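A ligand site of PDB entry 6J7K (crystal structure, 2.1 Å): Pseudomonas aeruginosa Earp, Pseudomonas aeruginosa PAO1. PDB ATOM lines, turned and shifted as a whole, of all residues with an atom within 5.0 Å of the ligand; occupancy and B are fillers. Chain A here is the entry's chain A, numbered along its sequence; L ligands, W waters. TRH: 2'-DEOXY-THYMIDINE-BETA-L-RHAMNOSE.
Gly 37 touches the ligand (CA to O3', 3.9 Å). Ile 67 touches the ligand (CG2 to O4', 3.8 Å). Tyr 131 touches the ligand (CE1 to O3, 3.0 Å). Phe 209 touches the ligand (CD1 to C5A, 3.5 Å). CB of Pro 235 touches C5A of the ligand, at 3.7 Å. Phe 270 touches the ligand. C of Ala 272 touches O21 of the ligand (3.8 Å). Tyr 276 touches the ligand (CE1 to C5A, 3.6 Å). Gly 290 touches the ligand (C to O2P, 3.7 Å). Hydrophobic or aromatic side chains that line the ligand: Ile 67, Tyr 131, Phe 209, Tyr 211, Pro 235, Phe 270, Met 271 and Tyr 276. Of the 27 residues printed, 20 come within 4 Å of the ligand.
N of Met 271 lies within hydrogen-bond range of O41 of the ligand, 3.1 Å away. O of Met 271 lies within hydrogen-bond range of N31 of the ligand, at 2.4 Å. The backbone NH (N) of Asp 292 is in hydrogen-bond range of an oxygen (O2P) of the ligand (3.0 Å). O3' of the ligand lies within hydrogen-bond range of OD1 of Asp 292, 2.6 Å away. The guanidinium group of Arg 289 lies within salt-bridge range of an oxygen (O3P) of the ligand, at 2.7 Å. The backbone NH (N) of Ser 293 lies within hydrogen-bond range of an oxygen (O1P) of the ligand, 2.7 Å away. OG of Ser 293 is in hydrogen-bond range of O1P of the ligand (2.8 Å). O3P of the ligand sits at hydrogen-bond distance from OH of Tyr 211. An oxygen (O2P) of the ligand lies within hydrogen-bond range of the backbone NH (N) of Glu 291, 2.7 Å away. An oxygen (O2) of the ligand sits at hydrogen-bond distance from the backbone NH (N) of Asp 35 (3.2 Å). An oxygen (O2) of the ligand lies within hydrogen-bond range of the side-chain carboxylate (OD1) of Asp 35 (2.9 Å). O5 of the ligand lies within hydrogen-bond range of ND2 of Asn 32 (2.9 Å). The backbone NH of Gly 34 is in hydrogen-bond range of an oxygen (O1) of the ligand (3.1 Å). An oxygen (O21) of the ligand sits close to the backbone NH (N) of Gln 273 (3.4 Å). The side-chain amide nitrogen of Gln 273 lies within hydrogen-bond range of an oxygen (O3') of the ligand (3.1 Å). An oxygen (O4P) of the ligand is in hydrogen-bond range of the backbone NH (N) of Tyr 33 (3.1 Å).
Water W1 lies within hydrogen-bond range of OD1 of Asp 35 (2.9 Å), O of Gly 34 (3.2 Å) and O3 of the ligand (3.5 Å).
The side-chain carboxylate (OD2) of Asp 292 lies within salt-bridge range of the guanidinium group (NE) of Arg 41. O of Arg 289 sits at hydrogen-bond distance from OG of Ser 293, at 2.7 Å. The backbone carbonyl oxygen (O) of Arg 289 sits at hydrogen-bond distance from the backbone NH (N) of Phe 294 (3.5 Å). OD2 of Asp 35 is in hydrogen-bond range of OH of Tyr 131, 2.8 Å away. N of Gln 273 lies within hydrogen-bond range of O of Ile 67. The backbone carbonyl oxygen (O) of Gly 37 lies within hydrogen-bond range of the side-chain amide nitrogen (NE2) of Gln 273 (3.2 Å). The side-chain hydroxyl (OH) of Tyr 33 lies close to the guanidinium group (NE) of Arg 66 (3.2 Å).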
ATOM      1  N   ASP A  31      22.524  -9.763  16.824  1.00  0.00           N
ATOM      2  CA  ASP A  31      22.282  -9.677  18.259  1.00  0.00           C
ATOM      3  C   ASP A  31      21.451 -10.885  18.654  1.00  0.00           C
ATOM      4  O   ASP A  31      20.774 -11.490  17.819  1.00  0.00           O
ATOM      5  CB  ASP A  31      21.565  -8.369  18.634  1.00  0.00           C
ATOM      6  CG  ASP A  31      22.043  -7.811  19.958  1.00  0.00           C
ATOM      7  OD1 ASP A  31      22.504  -8.604  20.811  1.00  0.00           O
ATOM      8  OD2 ASP A  31      21.972  -6.582  20.145  1.00  0.00           O
ATOM      9  N   ASN A  32      21.510 -11.223  19.943  1.00  0.00           N
ATOM     10  CA  ASN A  32      20.777 -12.353  20.498  1.00  0.00           C
ATOM     11  C   ASN A  32      21.146 -13.657  19.794  1.00  0.00           C
ATOM     12  O   ASN A  32      22.189 -13.739  19.128  1.00  0.00           O
ATOM     13  CB  ASN A  32      19.272 -12.114  20.430  1.00  0.00           C
ATOM     14  CG  ASN A  32      18.879 -10.752  20.986  1.00  0.00           C
ATOM     15  OD1 ASN A  32      19.337 -10.344  22.049  1.00  0.00           O
ATOM     16  ND2 ASN A  32      18.021 -10.053  20.261  1.00  0.00           N
ATOM     17  N   TYR A  33      20.289 -14.671  19.911  1.00  0.00           N
ATOM     18  CA  TYR A  33      20.628 -16.010  19.436  1.00  0.00           C
ATOM     19  C   TYR A  33      19.641 -16.537  18.402  1.00  0.00           C
ATOM     20  O   TYR A  33      19.717 -17.718  18.037  1.00  0.00           O
ATOM     21  CB  TYR A  33      20.710 -16.970  20.623  1.00  0.00           C
ATOM     22  CG  TYR A  33      21.694 -16.533  21.682  1.00  0.00           C
ATOM     23  CD1 TYR A  33      23.064 -16.733  21.513  1.00  0.00           C
ATOM     24  CD2 TYR A  33      21.263 -15.911  22.846  1.00  0.00           C
ATOM     25  CE1 TYR A  33      23.966 -16.321  22.473  1.00  0.00           C
ATOM     26  CE2 TYR A  33      22.163 -15.498  23.820  1.00  0.00           C
ATOM     27  CZ  TYR A  33      23.515 -15.704  23.626  1.00  0.00           C
ATOM     28  OH  TYR A  33      24.413 -15.304  24.580  1.00  0.00           O
ATOM     29  N   GLY A  34      18.731 -15.703  17.905  1.00  0.00           N
ATOM     30  CA  GLY A  34      17.714 -16.149  16.971  1.00  0.00           C
ATOM     31  C   GLY A  34      18.201 -16.367  15.558  1.00  0.00           C
ATOM     32  O   GLY A  34      17.776 -17.319  14.892  1.00  0.00           O
ATOM     33  N   ASP A  35      19.053 -15.476  15.063  1.00  0.00           N
ATOM     34  CA  ASP A  35      19.528 -15.619  13.690  1.00  0.00           C
ATOM     35  C   ASP A  35      20.458 -16.821  13.551  1.00  0.00           C
ATOM     36  O   ASP A  35      20.367 -17.579  12.576  1.00  0.00           O
ATOM     37  CB  ASP A  35      20.196 -14.333  13.229  1.00  0.00           C
ATOM     38  CG  ASP A  35      19.189 -13.195  13.051  1.00  0.00           C
ATOM     39  OD1 ASP A  35      17.997 -13.405  13.382  1.00  0.00           O
ATOM     40  OD2 ASP A  35      19.586 -12.104  12.592  1.00  0.00           O
ATOM     41  N   GLY A  37      20.268 -19.240  15.735  1.00  0.00           N
ATOM     42  CA  GLY A  37      19.387 -20.347  16.103  1.00  0.00           C
ATOM     43  C   GLY A  37      18.625 -20.900  14.915  1.00  0.00           C
ATOM     44  O   GLY A  37      18.485 -22.116  14.762  1.00  0.00           O
ATOM     45  N   ARG A  41      19.338 -24.476  12.950  1.00  0.00           N
ATOM     46  CA  ARG A  41      18.250 -25.447  12.819  1.00  0.00           C
ATOM     47  C   ARG A  41      18.075 -25.865  11.360  1.00  0.00           C
ATOM     48  O   ARG A  41      17.894 -27.055  11.066  1.00  0.00           O
ATOM     49  CB  ARG A  41      16.943 -24.860  13.362  1.00  0.00           C
ATOM     50  CG  ARG A  41      15.759 -25.802  13.254  1.00  0.00           C
ATOM     51  CD  ARG A  41      14.498 -25.210  13.863  1.00  0.00           C
ATOM     52  NE  ARG A  41      14.727 -24.706  15.214  1.00  0.00           N
ATOM     53  CZ  ARG A  41      14.812 -25.465  16.300  1.00  0.00           C
ATOM     54  NH1 ARG A  41      14.705 -26.783  16.185  1.00  0.00           N
ATOM     55  NH2 ARG A  41      15.017 -24.927  17.484  1.00  0.00           N
ATOM     56  N   ARG A  66      26.614 -21.340  22.501  1.00  0.00           N
ATOM     57  CA  ARG A  66      25.659 -21.399  23.602  1.00  0.00           C
ATOM     58  C   ARG A  66      24.362 -22.110  23.218  1.00  0.00           C
ATOM     59  O   ARG A  66      23.719 -22.714  24.093  1.00  0.00           O
ATOM     60  CB  ARG A  66      25.342 -19.989  24.130  1.00  0.00           C
ATOM     61  CG  ARG A  66      25.156 -19.956  25.639  1.00  0.00           C
ATOM     62  CD  ARG A  66      25.195 -18.545  26.216  1.00  0.00           C
ATOM     63  NE  ARG A  66      23.870 -17.933  26.291  1.00  0.00           N
ATOM     64  CZ  ARG A  66      23.572 -16.893  27.072  1.00  0.00           C
ATOM     65  NH1 ARG A  66      24.504 -16.360  27.844  1.00  0.00           N
ATOM     66  NH2 ARG A  66      22.342 -16.397  27.082  1.00  0.00           N
ATOM     67  N   ILE A  67      23.976 -22.076  21.947  1.00  0.00           N
ATOM     68  CA  ILE A  67      22.835 -22.874  21.499  1.00  0.00           C
ATOM     69  C   ILE A  67      23.240 -24.293  21.110  1.00  0.00           C
ATOM     70  O   ILE A  67      22.376 -25.173  21.023  1.00  0.00           O
ATOM     71  CB  ILE A  67      22.110 -22.195  20.322  1.00  0.00           C
ATOM     72  CG1 ILE A  67      23.035 -22.073  19.115  1.00  0.00           C
ATOM     73  CG2 ILE A  67      21.566 -20.835  20.737  1.00  0.00           C
ATOM     74  CD1 ILE A  67      22.354 -21.517  17.888  1.00  0.00           C
ATOM     75  N   TYR A 131      13.106 -12.872   7.419  1.00  0.00           N
ATOM     76  CA  TYR A 131      12.478 -13.101   8.704  1.00  0.00           C
ATOM     77  C   TYR A 131      11.037 -13.565   8.499  1.00  0.00           C
ATOM     78  O   TYR A 131      10.385 -13.227   7.517  1.00  0.00           O
ATOM     79  CB  TYR A 131      12.514 -11.837   9.556  1.00  0.00           C
ATOM     80  CG  TYR A 131      13.904 -11.447  10.027  1.00  0.00           C
ATOM     81  CD1 TYR A 131      14.576 -12.219  10.952  1.00  0.00           C
ATOM     82  CD2 TYR A 131      14.528 -10.304   9.545  1.00  0.00           C
ATOM     83  CE1 TYR A 131      15.850 -11.873  11.378  1.00  0.00           C
ATOM     84  CE2 TYR A 131      15.801  -9.948   9.970  1.00  0.00           C
ATOM     85  CZ  TYR A 131      16.448 -10.744  10.893  1.00  0.00           C
ATOM     86  OH  TYR A 131      17.714 -10.399  11.325  1.00  0.00           O
ATOM     87  N   PHE A 209      10.820 -16.626  28.707  1.00  0.00           N
ATOM     88  CA  PHE A 209      11.892 -16.278  27.791  1.00  0.00           C
ATOM     89  C   PHE A 209      11.472 -15.011  27.067  1.00  0.00           C
ATOM     90  O   PHE A 209      10.575 -15.051  26.212  1.00  0.00           O
ATOM     91  CB  PHE A 209      12.176 -17.410  26.793  1.00  0.00           C
ATOM     92  CG  PHE A 209      13.361 -17.154  25.907  1.00  0.00           C
ATOM     93  CD1 PHE A 209      14.564 -16.735  26.428  1.00  0.00           C
ATOM     94  CD2 PHE A 209      13.258 -17.355  24.531  1.00  0.00           C
ATOM     95  CE1 PHE A 209      15.664 -16.512  25.610  1.00  0.00           C
ATOM     96  CE2 PHE A 209      14.353 -17.135  23.704  1.00  0.00           C
ATOM     97  CZ  PHE A 209      15.553 -16.715  24.240  1.00  0.00           C
ATOM     98  N   TYR A 211      12.567 -10.366  26.659  1.00  0.00           N
ATOM     99  CA  TYR A 211      13.527  -9.295  26.843  1.00  0.00           C
ATOM    100  C   TYR A 211      13.186  -8.559  28.141  1.00  0.00           C
ATOM    101  O   TYR A 211      12.377  -9.024  28.950  1.00  0.00           O
ATOM    102  CB  TYR A 211      13.512  -8.359  25.628  1.00  0.00           C
ATOM    103  CG  TYR A 211      13.572  -9.080  24.301  1.00  0.00           C
ATOM    104  CD1 TYR A 211      14.770  -9.594  23.817  1.00  0.00           C
ATOM    105  CD2 TYR A 211      12.435  -9.219  23.515  1.00  0.00           C
ATOM    106  CE1 TYR A 211      14.831 -10.249  22.599  1.00  0.00           C
ATOM    107  CE2 TYR A 211      12.489  -9.876  22.288  1.00  0.00           C
ATOM    108  CZ  TYR A 211      13.688 -10.385  21.841  1.00  0.00           C
ATOM    109  OH  TYR A 211      13.753 -11.028  20.629  1.00  0.00           O
ATOM    110  N   PRO A 235      14.978 -19.626  32.208  1.00  0.00           N
ATOM    111  CA  PRO A 235      16.343 -19.857  31.737  1.00  0.00           C
ATOM    112  C   PRO A 235      17.166 -18.580  31.868  1.00  0.00           C
ATOM    113  O   PRO A 235      16.653 -17.474  31.723  1.00  0.00           O
ATOM    114  CB  PRO A 235      16.158 -20.258  30.268  1.00  0.00           C
ATOM    115  CG  PRO A 235      14.726 -20.696  30.163  1.00  0.00           C
ATOM    116  CD  PRO A 235      13.980 -19.852  31.145  1.00  0.00           C
ATOM    117  N   PRO A 269      19.364 -23.204  33.666  1.00  0.00           N
ATOM    118  CA  PRO A 269      20.492 -22.842  32.794  1.00  0.00           C
ATOM    119  C   PRO A 269      20.015 -22.576  31.381  1.00  0.00           C
ATOM    120  O   PRO A 269      18.898 -22.934  30.983  1.00  0.00           O
ATOM    121  CB  PRO A 269      21.407 -24.069  32.871  1.00  0.00           C
ATOM    122  CG  PRO A 269      20.492 -25.202  33.157  1.00  0.00           C
ATOM    123  CD  PRO A 269      19.395 -24.629  34.041  1.00  0.00           C
ATOM    124  N   PHE A 270      20.874 -21.926  30.603  1.00  0.00           N
ATOM    125  CA  PHE A 270      20.647 -21.787  29.169  1.00  0.00           C
ATOM    126  C   PHE A 270      20.996 -23.125  28.537  1.00  0.00           C
ATOM    127  O   PHE A 270      22.168 -23.472  28.407  1.00  0.00           O
ATOM    128  CB  PHE A 270      21.483 -20.644  28.587  1.00  0.00           C
ATOM    129  CG  PHE A 270      21.046 -20.224  27.208  1.00  0.00           C
ATOM    130  CD1 PHE A 270      20.073 -19.253  27.047  1.00  0.00           C
ATOM    131  CD2 PHE A 270      21.603 -20.811  26.084  1.00  0.00           C
ATOM    132  CE1 PHE A 270      19.682 -18.861  25.780  1.00  0.00           C
ATOM    133  CE2 PHE A 270      21.198 -20.422  24.815  1.00  0.00           C
ATOM    134  CZ  PHE A 270      20.244 -19.446  24.664  1.00  0.00           C
ATOM    135  N   MET A 271      19.973 -23.891  28.186  1.00  0.00           N
ATOM    136  CA  MET A 271      20.155 -25.284  27.798  1.00  0.00           C
ATOM    137  C   MET A 271      20.256 -25.461  26.297  1.00  0.00           C
ATOM    138  O   MET A 271      19.973 -24.525  25.532  1.00  0.00           O
ATOM    139  CB  MET A 271      18.996 -26.133  28.349  1.00  0.00           C
ATOM    140  CG  MET A 271      17.650 -25.756  27.759  1.00  0.00           C
ATOM    141  SD  MET A 271      16.141 -26.166  28.937  1.00  0.00           S
ATOM    142  CE  MET A 271      16.398 -24.782  30.278  1.00  0.00           C
ATOM    143  N   ALA A 272      20.664 -26.651  25.862  1.00  0.00           N
ATOM    144  CA  ALA A 272      20.759 -26.950  24.445  1.00  0.00           C
ATOM    145  C   ALA A 272      19.406 -26.740  23.764  1.00  0.00           C
ATOM    146  O   ALA A 272      18.345 -26.808  24.392  1.00  0.00           O
ATOM    147  CB  ALA A 272      21.249 -28.385  24.224  1.00  0.00           C
ATOM    148  N   GLN A 273      19.467 -26.457  22.466  1.00  0.00           N
ATOM    149  CA  GLN A 273      18.266 -26.100  21.717  1.00  0.00           C
ATOM    150  C   GLN A 273      17.190 -27.181  21.816  1.00  0.00           C
ATOM    151  O   GLN A 273      16.012 -26.874  22.037  1.00  0.00           O
ATOM    152  CB  GLN A 273      18.633 -25.842  20.259  1.00  0.00           C
ATOM    153  CG  GLN A 273      17.772 -24.815  19.555  1.00  0.00           C
ATOM    154  CD  GLN A 273      18.258 -24.532  18.145  1.00  0.00           C
ATOM    155  OE1 GLN A 273      18.761 -25.424  17.471  1.00  0.00           O
ATOM    156  NE2 GLN A 273      18.130 -23.284  17.706  1.00  0.00           N
ATOM    157  N   TYR A 276      15.561 -27.214  25.171  1.00  0.00           N
ATOM    158  CA  TYR A 276      14.595 -26.130  25.302  1.00  0.00           C
ATOM    159  C   TYR A 276      13.237 -26.538  24.737  1.00  0.00           C
ATOM    160  O   TYR A 276      12.197 -26.146  25.276  1.00  0.00           O
ATOM    161  CB  TYR A 276      15.119 -24.870  24.587  1.00  0.00           C
ATOM    162  CG  TYR A 276      14.202 -23.670  24.693  1.00  0.00           C
ATOM    163  CD1 TYR A 276      13.830 -23.162  25.930  1.00  0.00           C
ATOM    164  CD2 TYR A 276      13.719 -23.040  23.557  1.00  0.00           C
ATOM    165  CE1 TYR A 276      12.995 -22.061  26.039  1.00  0.00           C
ATOM    166  CE2 TYR A 276      12.894 -21.941  23.647  1.00  0.00           C
ATOM    167  CZ  TYR A 276      12.525 -21.452  24.886  1.00  0.00           C
ATOM    168  OH  TYR A 276      11.706 -20.351  24.984  1.00  0.00           O
ATOM    169  N   ARG A 289       9.816 -15.408  22.542  1.00  0.00           N
ATOM    170  CA  ARG A 289      10.237 -14.136  21.959  1.00  0.00           C
ATOM    171  C   ARG A 289      10.876 -14.395  20.598  1.00  0.00           C
ATOM    172  O   ARG A 289      11.142 -15.537  20.227  1.00  0.00           O
ATOM    173  CB  ARG A 289      11.222 -13.420  22.887  1.00  0.00           C
ATOM    174  CG  ARG A 289      12.654 -13.923  22.747  1.00  0.00           C
ATOM    175  CD  ARG A 289      13.575 -13.341  23.815  1.00  0.00           C
ATOM    176  NE  ARG A 289      14.983 -13.482  23.429  1.00  0.00           N
ATOM    177  CZ  ARG A 289      16.003 -13.335  24.258  1.00  0.00           C
ATOM    178  NH1 ARG A 289      15.796 -13.052  25.534  1.00  0.00           N
ATOM    179  NH2 ARG A 289      17.247 -13.479  23.815  1.00  0.00           N
ATOM    180  N   GLY A 290      11.120 -13.312  19.875  1.00  0.00           N
ATOM    181  CA  GLY A 290      11.920 -13.393  18.667  1.00  0.00           C
ATOM    182  C   GLY A 290      11.279 -14.221  17.574  1.00  0.00           C
ATOM    183  O   GLY A 290      10.091 -14.088  17.270  1.00  0.00           O
ATOM    184  N   GLU A 291      12.082 -15.107  16.974  1.00  0.00           N
ATOM    185  CA  GLU A 291      11.667 -15.862  15.791  1.00  0.00           C
ATOM    186  C   GLU A 291      11.603 -17.356  16.063  1.00  0.00           C
ATOM    187  O   GLU A 291      10.555 -17.976  15.844  1.00  0.00           O
ATOM    188  CB  GLU A 291      12.623 -15.576  14.622  1.00  0.00           C
ATOM    189  CG  GLU A 291      12.647 -14.121  14.188  1.00  0.00           C
ATOM    190  CD  GLU A 291      11.855 -13.884  12.917  1.00  0.00           C
ATOM    191  OE1 GLU A 291      12.035 -14.651  11.941  1.00  0.00           O
ATOM    192  OE2 GLU A 291      11.051 -12.919  12.888  1.00  0.00           O
ATOM    193  N   ASP A 292      12.701 -17.973  16.512  1.00  0.00           N
ATOM    194  CA  ASP A 292      12.733 -19.422  16.631  1.00  0.00           C
ATOM    195  C   ASP A 292      11.866 -19.910  17.786  1.00  0.00           C
ATOM    196  O   ASP A 292      10.962 -20.718  17.598  1.00  0.00           O
ATOM    197  CB  ASP A 292      14.183 -19.904  16.773  1.00  0.00           C
ATOM    198  CG  ASP A 292      14.284 -21.422  16.760  1.00  0.00           C
ATOM    199  OD1 ASP A 292      14.480 -22.021  17.841  1.00  0.00           O
ATOM    200  OD2 ASP A 292      14.131 -22.020  15.678  1.00  0.00           O
ATOM    201  N   SER A 293      12.130 -19.399  18.998  1.00  0.00           N
ATOM    202  CA  SER A 293      11.332 -19.826  20.152  1.00  0.00           C
ATOM    203  C   SER A 293       9.861 -19.470  20.005  1.00  0.00           C
ATOM    204  O   SER A 293       9.022 -20.105  20.640  1.00  0.00           O
ATOM    205  CB  SER A 293      11.884 -19.200  21.432  1.00  0.00           C
ATOM    206  OG  SER A 293      11.536 -17.833  21.519  1.00  0.00           O
ATOM    207  N   PHE A 294       9.552 -18.464  19.192  1.00  0.00           N
ATOM    208  CA  PHE A 294       8.164 -18.133  18.918  1.00  0.00           C
ATOM    209  C   PHE A 294       7.465 -19.271  18.166  1.00  0.00           C
ATOM    210  O   PHE A 294       6.306 -19.585  18.450  1.00  0.00           O
ATOM    211  CB  PHE A 294       8.102 -16.820  18.130  1.00  0.00           C
ATOM    212  CG  PHE A 294       6.749 -16.503  17.560  1.00  0.00           C
ATOM    213  CD1 PHE A 294       6.604 -16.312  16.193  1.00  0.00           C
ATOM    214  CD2 PHE A 294       5.637 -16.370  18.375  1.00  0.00           C
ATOM    215  CE1 PHE A 294       5.373 -16.013  15.654  1.00  0.00           C
ATOM    216  CE2 PHE A 294       4.406 -16.071  17.836  1.00  0.00           C
ATOM    217  CZ  PHE A 294       4.263 -15.890  16.469  1.00  0.00           C
ATOM    218  N   TYR A 309      10.550  -7.742  19.967  1.00  0.00           N
ATOM    219  CA  TYR A 309      11.352  -6.573  20.301  1.00  0.00           C
ATOM    220  C   TYR A 309      10.904  -5.363  19.499  1.00  0.00           C
ATOM    221  O   TYR A 309      10.565  -5.472  18.317  1.00  0.00           O
ATOM    222  CB  TYR A 309      12.830  -6.859  20.052  1.00  0.00           C
ATOM    223  CG  TYR A 309      13.781  -5.923  20.762  1.00  0.00           C
ATOM    224  CD1 TYR A 309      14.117  -6.131  22.086  1.00  0.00           C
ATOM    225  CD2 TYR A 309      14.343  -4.843  20.102  1.00  0.00           C
ATOM    226  CE1 TYR A 309      14.990  -5.284  22.749  1.00  0.00           C
ATOM    227  CE2 TYR A 309      15.217  -3.988  20.750  1.00  0.00           C
ATOM    228  CZ  TYR A 309      15.532  -4.209  22.079  1.00  0.00           C
ATOM    229  OH  TYR A 309      16.402  -3.366  22.719  1.00  0.00           O
ATOM    230  N   GLN A 311      10.905  -1.947  17.354  1.00  0.00           N
ATOM    231  CA  GLN A 311      11.670  -1.591  16.166  1.00  0.00           C
ATOM    232  C   GLN A 311      11.546  -0.096  15.889  1.00  0.00           C
ATOM    233  O   GLN A 311      11.015   0.667  16.702  1.00  0.00           O
ATOM    234  CB  GLN A 311      11.200  -2.428  14.967  1.00  0.00           C
ATOM    235  CG  GLN A 311      11.407  -3.925  15.136  1.00  0.00           C
ATOM    236  CD  GLN A 311      12.871  -4.302  15.205  1.00  0.00           C
ATOM    237  OE1 GLN A 311      13.734  -3.608  14.676  1.00  0.00           O
ATOM    238  NE2 GLN A 311      13.157  -5.413  15.874  1.00  0.00           N
HETATM  239  O4P TRH L   1      17.373 -14.689  20.913  1.00  0.00           O
HETATM  240  P2  TRH L   1      16.174 -14.046  20.242  1.00  0.00           P
HETATM  241  O3P TRH L   1      15.767 -12.795  20.973  1.00  0.00           O
HETATM  242  O1  TRH L   1      16.583 -13.616  18.650  1.00  0.00           O
HETATM  243  C1  TRH L   1      15.775 -12.730  18.043  1.00  0.00           C
HETATM  244  C2  TRH L   1      15.817 -12.978  16.539  1.00  0.00           C
HETATM  245  O2  TRH L   1      17.209 -13.026  16.105  1.00  0.00           O
HETATM  246  C3  TRH L   1      15.081 -11.940  15.770  1.00  0.00           C
HETATM  247  O3  TRH L   1      15.375 -12.104  14.367  1.00  0.00           O
HETATM  248  C4  TRH L   1      15.435 -10.522  16.185  1.00  0.00           C
HETATM  249  O4  TRH L   1      14.512  -9.653  15.589  1.00  0.00           O
HETATM  250  C5  TRH L   1      15.379 -10.326  17.700  1.00  0.00           C
HETATM  251  O5  TRH L   1      16.190 -11.321  18.405  1.00  0.00           O
HETATM  252  C6  TRH L   1      15.858  -8.940  18.047  1.00  0.00           C
HETATM  253  OPP TRH L   1      14.918 -15.077  20.232  1.00  0.00           O
HETATM  254  P   TRH L   1      14.813 -16.442  19.241  1.00  0.00           P
HETATM  255  O1P TRH L   1      13.685 -17.326  19.729  1.00  0.00           O
HETATM  256  O2P TRH L   1      14.527 -16.020  17.780  1.00  0.00           O
HETATM  257  O5' TRH L   1      16.279 -17.279  19.309  1.00  0.00           O
HETATM  258  C5' TRH L   1      16.723 -17.811  20.535  1.00  0.00           C
HETATM  259  C4' TRH L   1      17.237 -19.222  20.230  1.00  0.00           C
HETATM  260  O4' TRH L   1      17.967 -19.819  21.557  1.00  0.00           O
HETATM  261  C3' TRH L   1      16.234 -19.998  19.941  1.00  0.00           C
HETATM  262  O3' TRH L   1      16.581 -20.846  18.780  1.00  0.00           O
HETATM  263  C2' TRH L   1      16.032 -20.890  21.200  1.00  0.00           C
HETATM  264  C1' TRH L   1      17.463 -21.004  21.740  1.00  0.00           C
HETATM  265  N11 TRH L   1      17.473 -21.305  23.204  1.00  0.00           N
HETATM  266  C21 TRH L   1      18.314 -22.446  23.700  1.00  0.00           C
HETATM  267  O21 TRH L   1      18.971 -23.106  22.898  1.00  0.00           O
HETATM  268  N31 TRH L   1      18.341 -22.764  25.169  1.00  0.00           N
HETATM  269  C41 TRH L   1      17.564 -21.974  26.087  1.00  0.00           C
HETATM  270  O41 TRH L   1      17.586 -22.206  27.214  1.00  0.00           O
HETATM  271  C51 TRH L   1      16.740 -20.842  25.581  1.00  0.00           C
HETATM  272  C5A TRH L   1      15.901 -19.988  26.589  1.00  0.00           C
HETATM  273  C61 TRH L   1      16.704 -20.515  24.116  1.00  0.00           C
HETATM  274  O   HOH W   1      15.817 -15.365  13.302  1.00  0.00           O
